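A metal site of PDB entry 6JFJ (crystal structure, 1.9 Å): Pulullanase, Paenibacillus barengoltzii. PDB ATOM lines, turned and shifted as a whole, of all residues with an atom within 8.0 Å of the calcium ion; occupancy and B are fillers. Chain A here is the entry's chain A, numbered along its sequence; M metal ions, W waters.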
ATOM      1  N   VAL A 122     -12.950   6.836  16.741  1.00  0.00           N
ATOM      2  CA  VAL A 122     -14.277   7.274  17.159  1.00  0.00           C
ATOM      3  C   VAL A 122     -14.964   8.011  16.015  1.00  0.00           C
ATOM      4  O   VAL A 122     -14.335   8.493  15.076  1.00  0.00           O
ATOM      5  CB  VAL A 122     -14.243   8.201  18.401  1.00  0.00           C
ATOM      6  CG1 VAL A 122     -13.708   7.479  19.635  1.00  0.00           C
ATOM      7  CG2 VAL A 122     -13.475   9.518  18.104  1.00  0.00           C
ATOM      8  N   GLY A 123     -16.297   8.113  16.129  1.00  0.00           N
ATOM      9  CA  GLY A 123     -17.070   8.951  15.235  1.00  0.00           C
ATOM     10  C   GLY A 123     -16.967  10.425  15.616  1.00  0.00           C
ATOM     11  O   GLY A 123     -16.273  10.807  16.560  1.00  0.00           O
ATOM     12  N   VAL A 124     -17.686  11.256  14.855  1.00  0.00           N
ATOM     13  CA  VAL A 124     -17.612  12.693  15.110  1.00  0.00           C
ATOM     14  C   VAL A 124     -18.005  12.963  16.549  1.00  0.00           C
ATOM     15  O   VAL A 124     -18.911  12.319  17.093  1.00  0.00           O
ATOM     16  CB  VAL A 124     -18.486  13.498  14.134  1.00  0.00           C
ATOM     17  CG1 VAL A 124     -19.987  13.315  14.435  1.00  0.00           C
ATOM     18  CG2 VAL A 124     -18.115  14.982  14.209  1.00  0.00           C
ATOM     19  N   ASN A 125     -17.271  13.869  17.188  1.00  0.00           N
ATOM     20  CA  ASN A 125     -17.475  14.263  18.580  1.00  0.00           C
ATOM     21  C   ASN A 125     -17.341  13.108  19.578  1.00  0.00           C
ATOM     22  O   ASN A 125     -17.726  13.262  20.741  1.00  0.00           O
ATOM     23  CB  ASN A 125     -18.827  14.960  18.756  1.00  0.00           C
ATOM     24  CG  ASN A 125     -18.768  16.406  18.362  1.00  0.00           C
ATOM     25  OD1 ASN A 125     -17.772  17.089  18.614  1.00  0.00           O
ATOM     26  ND2 ASN A 125     -19.822  16.885  17.697  1.00  0.00           N
ATOM     27  N   GLY A 126     -16.801  11.983  19.142  1.00  0.00           N
ATOM     28  CA  GLY A 126     -16.352  10.941  20.058  1.00  0.00           C
ATOM     29  C   GLY A 126     -17.448  10.297  20.873  1.00  0.00           C
ATOM     30  O   GLY A 126     -17.196   9.900  22.018  1.00  0.00           O
ATOM     31  N   TYR A 215      -4.974  14.771  21.635  1.00  0.00           N
ATOM     32  CA  TYR A 215      -5.984  13.757  21.936  1.00  0.00           C
ATOM     33  C   TYR A 215      -7.376  14.364  21.774  1.00  0.00           C
ATOM     34  O   TYR A 215      -7.546  15.586  21.659  1.00  0.00           O
ATOM     35  CB  TYR A 215      -5.797  13.221  23.369  1.00  0.00           C
ATOM     36  CG  TYR A 215      -5.866  14.342  24.375  1.00  0.00           C
ATOM     37  CD1 TYR A 215      -7.093  14.818  24.824  1.00  0.00           C
ATOM     38  CD2 TYR A 215      -4.712  14.974  24.832  1.00  0.00           C
ATOM     39  CE1 TYR A 215      -7.179  15.877  25.691  1.00  0.00           C
ATOM     40  CE2 TYR A 215      -4.785  16.038  25.717  1.00  0.00           C
ATOM     41  CZ  TYR A 215      -6.025  16.487  26.138  1.00  0.00           C
ATOM     42  OH  TYR A 215      -6.136  17.545  27.000  1.00  0.00           O
ATOM     43  N   ASP A 216      -8.401  13.515  21.802  1.00  0.00           N
ATOM     44  CA  ASP A 216      -9.767  13.975  21.545  1.00  0.00           C
ATOM     45  C   ASP A 216     -10.316  14.693  22.768  1.00  0.00           C
ATOM     46  O   ASP A 216     -10.520  14.081  23.818  1.00  0.00           O
ATOM     47  CB  ASP A 216     -10.665  12.802  21.163  1.00  0.00           C
ATOM     48  CG  ASP A 216     -12.076  13.247  20.812  1.00  0.00           C
ATOM     49  OD1 ASP A 216     -12.235  14.411  20.420  1.00  0.00           O
ATOM     50  OD2 ASP A 216     -13.025  12.432  20.907  1.00  0.00           O
ATOM     51  N   TYR A 217     -10.558  16.003  22.645  1.00  0.00           N
ATOM     52  CA  TYR A 217     -11.151  16.757  23.734  1.00  0.00           C
ATOM     53  C   TYR A 217     -12.622  17.053  23.436  1.00  0.00           C
ATOM     54  O   TYR A 217     -13.109  16.828  22.330  1.00  0.00           O
ATOM     55  CB  TYR A 217     -10.351  18.035  24.023  1.00  0.00           C
ATOM     56  CG  TYR A 217     -10.064  18.970  22.873  1.00  0.00           C
ATOM     57  CD1 TYR A 217     -11.004  19.913  22.470  1.00  0.00           C
ATOM     58  CD2 TYR A 217      -8.818  18.973  22.246  1.00  0.00           C
ATOM     59  CE1 TYR A 217     -10.736  20.803  21.447  1.00  0.00           C
ATOM     60  CE2 TYR A 217      -8.523  19.878  21.228  1.00  0.00           C
ATOM     61  CZ  TYR A 217      -9.504  20.788  20.822  1.00  0.00           C
ATOM     62  OH  TYR A 217      -9.259  21.687  19.824  1.00  0.00           O
ATOM     63  N   SER A 218     -13.317  17.558  24.444  1.00  0.00           N
ATOM     64  CA  SER A 218     -14.776  17.412  24.472  1.00  0.00           C
ATOM     65  C   SER A 218     -15.493  18.291  23.445  1.00  0.00           C
ATOM     66  O   SER A 218     -15.016  19.366  23.053  1.00  0.00           O
ATOM     67  CB  SER A 218     -15.306  17.751  25.866  1.00  0.00           C
ATOM     68  OG  SER A 218     -15.465  19.148  25.992  1.00  0.00           O
ATOM     69  N   GLN A 219     -16.684  17.838  23.056  1.00  0.00           N
ATOM     70  CA  GLN A 219     -17.557  18.580  22.151  1.00  0.00           C
ATOM     71  C   GLN A 219     -17.960  19.918  22.753  1.00  0.00           C
ATOM     72  O   GLN A 219     -18.196  20.884  22.010  1.00  0.00           O
ATOM     73  CB  GLN A 219     -18.788  17.727  21.822  1.00  0.00           C
ATOM     74  CG  GLN A 219     -19.906  18.460  21.108  1.00  0.00           C
ATOM     75  CD  GLN A 219     -21.157  17.602  20.956  1.00  0.00           C
ATOM     76  OE1 GLN A 219     -21.184  16.421  21.353  1.00  0.00           O
ATOM     77  NE2 GLN A 219     -22.200  18.180  20.381  1.00  0.00           N
ATOM     78  N   GLU A 220     -18.012  20.003  24.076  1.00  0.00           N
ATOM     79  CA  GLU A 220     -18.295  21.272  24.747  1.00  0.00           C
ATOM     80  C   GLU A 220     -17.206  22.301  24.481  1.00  0.00           C
ATOM     81  O   GLU A 220     -17.461  23.508  24.535  1.00  0.00           O
ATOM     82  CB  GLU A 220     -18.461  21.032  26.246  1.00  0.00           C
ATOM     83  CG  GLU A 220     -18.950  22.217  27.048  1.00  0.00           C
ATOM     84  CD  GLU A 220     -19.096  21.888  28.524  1.00  0.00           C
ATOM     85  OE1 GLU A 220     -18.553  22.642  29.363  1.00  0.00           O
ATOM     86  OE2 GLU A 220     -19.742  20.869  28.847  1.00  0.00           O
ATOM     87  N   SER A 221     -15.975  21.856  24.205  1.00  0.00           N
ATOM     88  CA  SER A 221     -14.879  22.786  23.938  1.00  0.00           C
ATOM     89  C   SER A 221     -14.842  23.216  22.473  1.00  0.00           C
ATOM     90  O   SER A 221     -14.771  24.411  22.169  1.00  0.00           O
ATOM     91  CB  SER A 221     -13.544  22.161  24.345  1.00  0.00           C
ATOM     92  OG  SER A 221     -13.514  21.831  25.716  1.00  0.00           O
ATOM     93  N   VAL A 222     -14.866  22.240  21.565  1.00  0.00           N
ATOM     94  CA  VAL A 222     -14.988  22.483  20.131  1.00  0.00           C
ATOM     95  C   VAL A 222     -15.960  21.456  19.590  1.00  0.00           C
ATOM     96  O   VAL A 222     -15.739  20.244  19.756  1.00  0.00           O
ATOM     97  CB  VAL A 222     -13.645  22.389  19.384  1.00  0.00           C
ATOM     98  CG1 VAL A 222     -13.867  22.294  17.869  1.00  0.00           C
ATOM     99  CG2 VAL A 222     -12.727  23.589  19.710  1.00  0.00           C
ATOM    100  N   ASP A 223     -17.043  21.917  18.962  1.00  0.00           N
ATOM    101  CA  ASP A 223     -18.029  21.024  18.361  1.00  0.00           C
ATOM    102  C   ASP A 223     -17.532  20.622  16.974  1.00  0.00           C
ATOM    103  O   ASP A 223     -17.517  21.440  16.051  1.00  0.00           O
ATOM    104  CB  ASP A 223     -19.396  21.703  18.286  1.00  0.00           C
ATOM    105  CG  ASP A 223     -20.509  20.723  17.915  1.00  0.00           C
ATOM    106  OD1 ASP A 223     -20.233  19.735  17.214  1.00  0.00           O
ATOM    107  OD2 ASP A 223     -21.658  20.959  18.339  1.00  0.00           O
ATOM    108  N   GLU A 224     -17.141  19.346  16.833  1.00  0.00           N
ATOM    109  CA  GLU A 224     -16.547  18.857  15.590  1.00  0.00           C
ATOM    110  C   GLU A 224     -17.545  18.778  14.449  1.00  0.00           C
ATOM    111  O   GLU A 224     -17.116  18.567  13.297  1.00  0.00           O
ATOM    112  CB  GLU A 224     -15.938  17.478  15.815  1.00  0.00           C
ATOM    113  CG  GLU A 224     -14.873  17.415  16.913  1.00  0.00           C
ATOM    114  CD  GLU A 224     -14.371  15.994  17.118  1.00  0.00           C
ATOM    115  OE1 GLU A 224     -14.838  15.112  16.377  1.00  0.00           O
ATOM    116  OE2 GLU A 224     -13.515  15.766  17.992  1.00  0.00           O
ATOM    117  N   ASP A 237      -9.637  19.505  28.115  1.00  0.00           N
ATOM    118  CA  ASP A 237     -10.877  18.867  28.561  1.00  0.00           C
ATOM    119  C   ASP A 237     -10.948  17.479  27.929  1.00  0.00           C
ATOM    120  O   ASP A 237     -11.624  17.294  26.909  1.00  0.00           O
ATOM    121  CB  ASP A 237     -12.094  19.701  28.150  1.00  0.00           C
ATOM    122  CG  ASP A 237     -11.949  21.175  28.513  1.00  0.00           C
ATOM    123  OD1 ASP A 237     -11.748  21.471  29.705  1.00  0.00           O
ATOM    124  OD2 ASP A 237     -12.047  22.036  27.601  1.00  0.00           O
ATOM    125  N   GLN A 239     -11.667  13.813  26.576  1.00  0.00           N
ATOM    126  CA  GLN A 239     -12.820  12.944  26.365  1.00  0.00           C
ATOM    127  C   GLN A 239     -12.410  11.548  25.935  1.00  0.00           C
ATOM    128  O   GLN A 239     -12.862  10.568  26.536  1.00  0.00           O
ATOM    129  CB  GLN A 239     -13.763  13.573  25.322  1.00  0.00           C
ATOM    130  CG  GLN A 239     -15.118  12.865  25.169  1.00  0.00           C
ATOM    131  CD  GLN A 239     -15.857  13.261  23.884  1.00  0.00           C
ATOM    132  OE1 GLN A 239     -15.492  14.225  23.208  1.00  0.00           O
ATOM    133  NE2 GLN A 239     -16.895  12.497  23.548  1.00  0.00           N
ATOM    134  N   ASN A 240     -11.561  11.417  24.917  1.00  0.00           N
ATOM    135  CA  ASN A 240     -11.068  10.107  24.501  1.00  0.00           C
ATOM    136  C   ASN A 240      -9.536  10.148  24.440  1.00  0.00           C
ATOM    137  O   ASN A 240      -8.963  10.714  23.502  1.00  0.00           O
ATOM    138  CB  ASN A 240     -11.686   9.678  23.166  1.00  0.00           C
ATOM    139  CG  ASN A 240     -13.196   9.486  23.275  1.00  0.00           C
ATOM    140  OD1 ASN A 240     -13.671   8.618  24.002  1.00  0.00           O
ATOM    141  ND2 ASN A 240     -13.954  10.316  22.552  1.00  0.00           N
ATOM    142  N   VAL A 243      -7.306   8.577  21.124  1.00  0.00           N
ATOM    143  CA  VAL A 243      -7.680   8.877  19.738  1.00  0.00           C
ATOM    144  C   VAL A 243      -7.394  10.368  19.514  1.00  0.00           C
ATOM    145  O   VAL A 243      -7.475  11.163  20.453  1.00  0.00           O
ATOM    146  CB  VAL A 243      -9.140   8.498  19.472  1.00  0.00           C
ATOM    147  CG1 VAL A 243     -10.070   9.392  20.228  1.00  0.00           C
ATOM    148  CG2 VAL A 243      -9.485   8.508  17.970  1.00  0.00           C
ATOM    149  N   PRO A 244      -7.021  10.778  18.299  1.00  0.00           N
ATOM    150  CA  PRO A 244      -6.756  12.201  18.079  1.00  0.00           C
ATOM    151  C   PRO A 244      -8.040  13.025  18.119  1.00  0.00           C
ATOM    152  O   PRO A 244      -9.151  12.505  18.020  1.00  0.00           O
ATOM    153  CB  PRO A 244      -6.124  12.253  16.684  1.00  0.00           C
ATOM    154  CG  PRO A 244      -5.604  10.886  16.426  1.00  0.00           C
ATOM    155  CD  PRO A 244      -6.587   9.972  17.140  1.00  0.00           C
ATOM    156  N   GLU A 245      -7.849  14.339  18.280  1.00  0.00           N
ATOM    157  CA  GLU A 245      -8.948  15.292  18.213  1.00  0.00           C
ATOM    158  C   GLU A 245      -9.476  15.392  16.787  1.00  0.00           C
ATOM    159  O   GLU A 245      -8.710  15.528  15.834  1.00  0.00           O
ATOM    160  CB  GLU A 245      -8.464  16.671  18.694  1.00  0.00           C
ATOM    161  CG  GLU A 245      -9.324  17.852  18.234  1.00  0.00           C
ATOM    162  CD  GLU A 245     -10.748  17.809  18.784  1.00  0.00           C
ATOM    163  OE1 GLU A 245     -11.010  17.062  19.754  1.00  0.00           O
ATOM    164  OE2 GLU A 245     -11.598  18.539  18.252  1.00  0.00           O
ATOM    165  N   GLY A 246     -10.811  15.325  16.658  1.00  0.00           N
ATOM    166  CA  GLY A 246     -11.429  15.311  15.341  1.00  0.00           C
ATOM    167  C   GLY A 246     -11.343  16.637  14.585  1.00  0.00           C
ATOM    168  O   GLY A 246     -11.224  16.634  13.361  1.00  0.00           O
ATOM    169  N   SER A 247     -11.406  17.767  15.295  1.00  0.00           N
ATOM    170  CA  SER A 247     -11.397  19.047  14.606  1.00  0.00           C
ATOM    171  C   SER A 247     -10.067  19.369  13.930  1.00  0.00           C
ATOM    172  O   SER A 247     -10.018  20.286  13.102  1.00  0.00           O
ATOM    173  CB  SER A 247     -11.772  20.184  15.569  1.00  0.00           C
ATOM    174  OG  SER A 247     -10.746  20.443  16.521  1.00  0.00           O
ATOM    175  N   TYR A 248      -8.985  18.644  14.244  1.00  0.00           N
ATOM    176  CA  TYR A 248      -7.731  18.862  13.543  1.00  0.00           C
ATOM    177  C   TYR A 248      -7.611  17.991  12.301  1.00  0.00           C
ATOM    178  O   TYR A 248      -6.570  18.017  11.632  1.00  0.00           O
ATOM    179  CB  TYR A 248      -6.529  18.636  14.483  1.00  0.00           C
ATOM    180  CG  TYR A 248      -6.544  19.527  15.724  1.00  0.00           C
ATOM    181  CD1 TYR A 248      -7.069  20.809  15.667  1.00  0.00           C
ATOM    182  CD2 TYR A 248      -6.040  19.072  16.943  1.00  0.00           C
ATOM    183  CE1 TYR A 248      -7.102  21.631  16.811  1.00  0.00           C
ATOM    184  CE2 TYR A 248      -6.064  19.877  18.085  1.00  0.00           C
ATOM    185  CZ  TYR A 248      -6.592  21.159  18.008  1.00  0.00           C
ATOM    186  OH  TYR A 248      -6.638  21.978  19.133  1.00  0.00           O
ATOM    187  N   PRO A 252     -13.725  15.123  10.204  1.00  0.00           N
ATOM    188  CA  PRO A 252     -13.976  14.528  11.528  1.00  0.00           C
ATOM    189  C   PRO A 252     -14.970  13.385  11.501  1.00  0.00           C
ATOM    190  O   PRO A 252     -15.057  12.637  12.478  1.00  0.00           O
ATOM    191  CB  PRO A 252     -14.531  15.712  12.343  1.00  0.00           C
ATOM    192  CG  PRO A 252     -14.287  16.933  11.516  1.00  0.00           C
ATOM    193  CD  PRO A 252     -14.239  16.495  10.093  1.00  0.00           C
ATOM    194  N   ARG A 258      -8.430  11.390  10.879  1.00  0.00           N
ATOM    195  CA  ARG A 258      -7.637  12.050  11.915  1.00  0.00           C
ATOM    196  C   ARG A 258      -6.416  11.221  12.304  1.00  0.00           C
ATOM    197  O   ARG A 258      -5.391  11.779  12.715  1.00  0.00           O
ATOM    198  CB  ARG A 258      -8.509  12.342  13.141  1.00  0.00           C
ATOM    199  CG  ARG A 258      -8.952  11.090  13.925  1.00  0.00           C
ATOM    200  CD  ARG A 258      -9.842  11.465  15.113  1.00  0.00           C
ATOM    201  NE  ARG A 258     -11.205  11.773  14.692  1.00  0.00           N
ATOM    202  CZ  ARG A 258     -12.176  12.129  15.530  1.00  0.00           C
ATOM    203  NH1 ARG A 258     -11.928  12.233  16.846  1.00  0.00           N
ATOM    204  NH2 ARG A 258     -13.386  12.395  15.070  1.00  0.00           N
HETATM  205 CA    CA M   1     -13.196  16.391  20.159  1.00  0.00          CA
HETATM  206  O   HOH W   1     -13.631  18.650  19.937  1.00  0.00           O
HETATM  207  O   HOH W   2     -15.184  15.438  20.801  1.00  0.00           O
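Water W2 bridges the side-chain amide oxygen of Gln 239 (2.7 Å) and the backbone carbonyl oxygen of Asn 125 (3.3 Å).
The calcium ion is bound by the side-chain carboxylate of Asp 216, the backbone carbonyl oxygen of Tyr 217, the side-chain carboxylate of Glu 224, water W2, water W1 and the side-chain carboxylate of Glu 245. The calcium ion has six donor atoms within binding distance.
N of Gln 239 lies within hydrogen-bond range of O of Asp 216. The side-chain amide nitrogen of Asn 240 is in hydrogen-bond range of the side-chain carboxylate of Asp 216 (2.8 Å). The backbone NH (N) of Asp 216 is in hydrogen-bond range of the backbone carbonyl oxygen (O) of Val 243. The side-chain hydroxyl (OH) of Tyr 248 is in hydrogen-bond range of the side-chain hydroxyl (OH) of Tyr 217 (2.7 Å). The side-chain carboxylate (OE2) of Glu 224 sits close to the backbone NH (N) of Gly 246 (3.0 Å). The side-chain carboxylate (OE1) of Glu 224 is in hydrogen-bond range of the backbone NH (N) of Asn 125 (2.8 Å). The guanidinium group (NH2) of Arg 258 is in salt-bridge range of the side-chain carboxylate (OE1) of Glu 224, at 3.3 Å. The side-chain carboxylate (OE2) of Glu 245 lies within hydrogen-bond range of the side-chain hydroxyl (OG) of Ser 247.
Of the 26 residues printed, 4 come within 4 Å of the calcium ion. Along chain A the residues within 4 Å of the calcium ion span positions 216 to 245.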
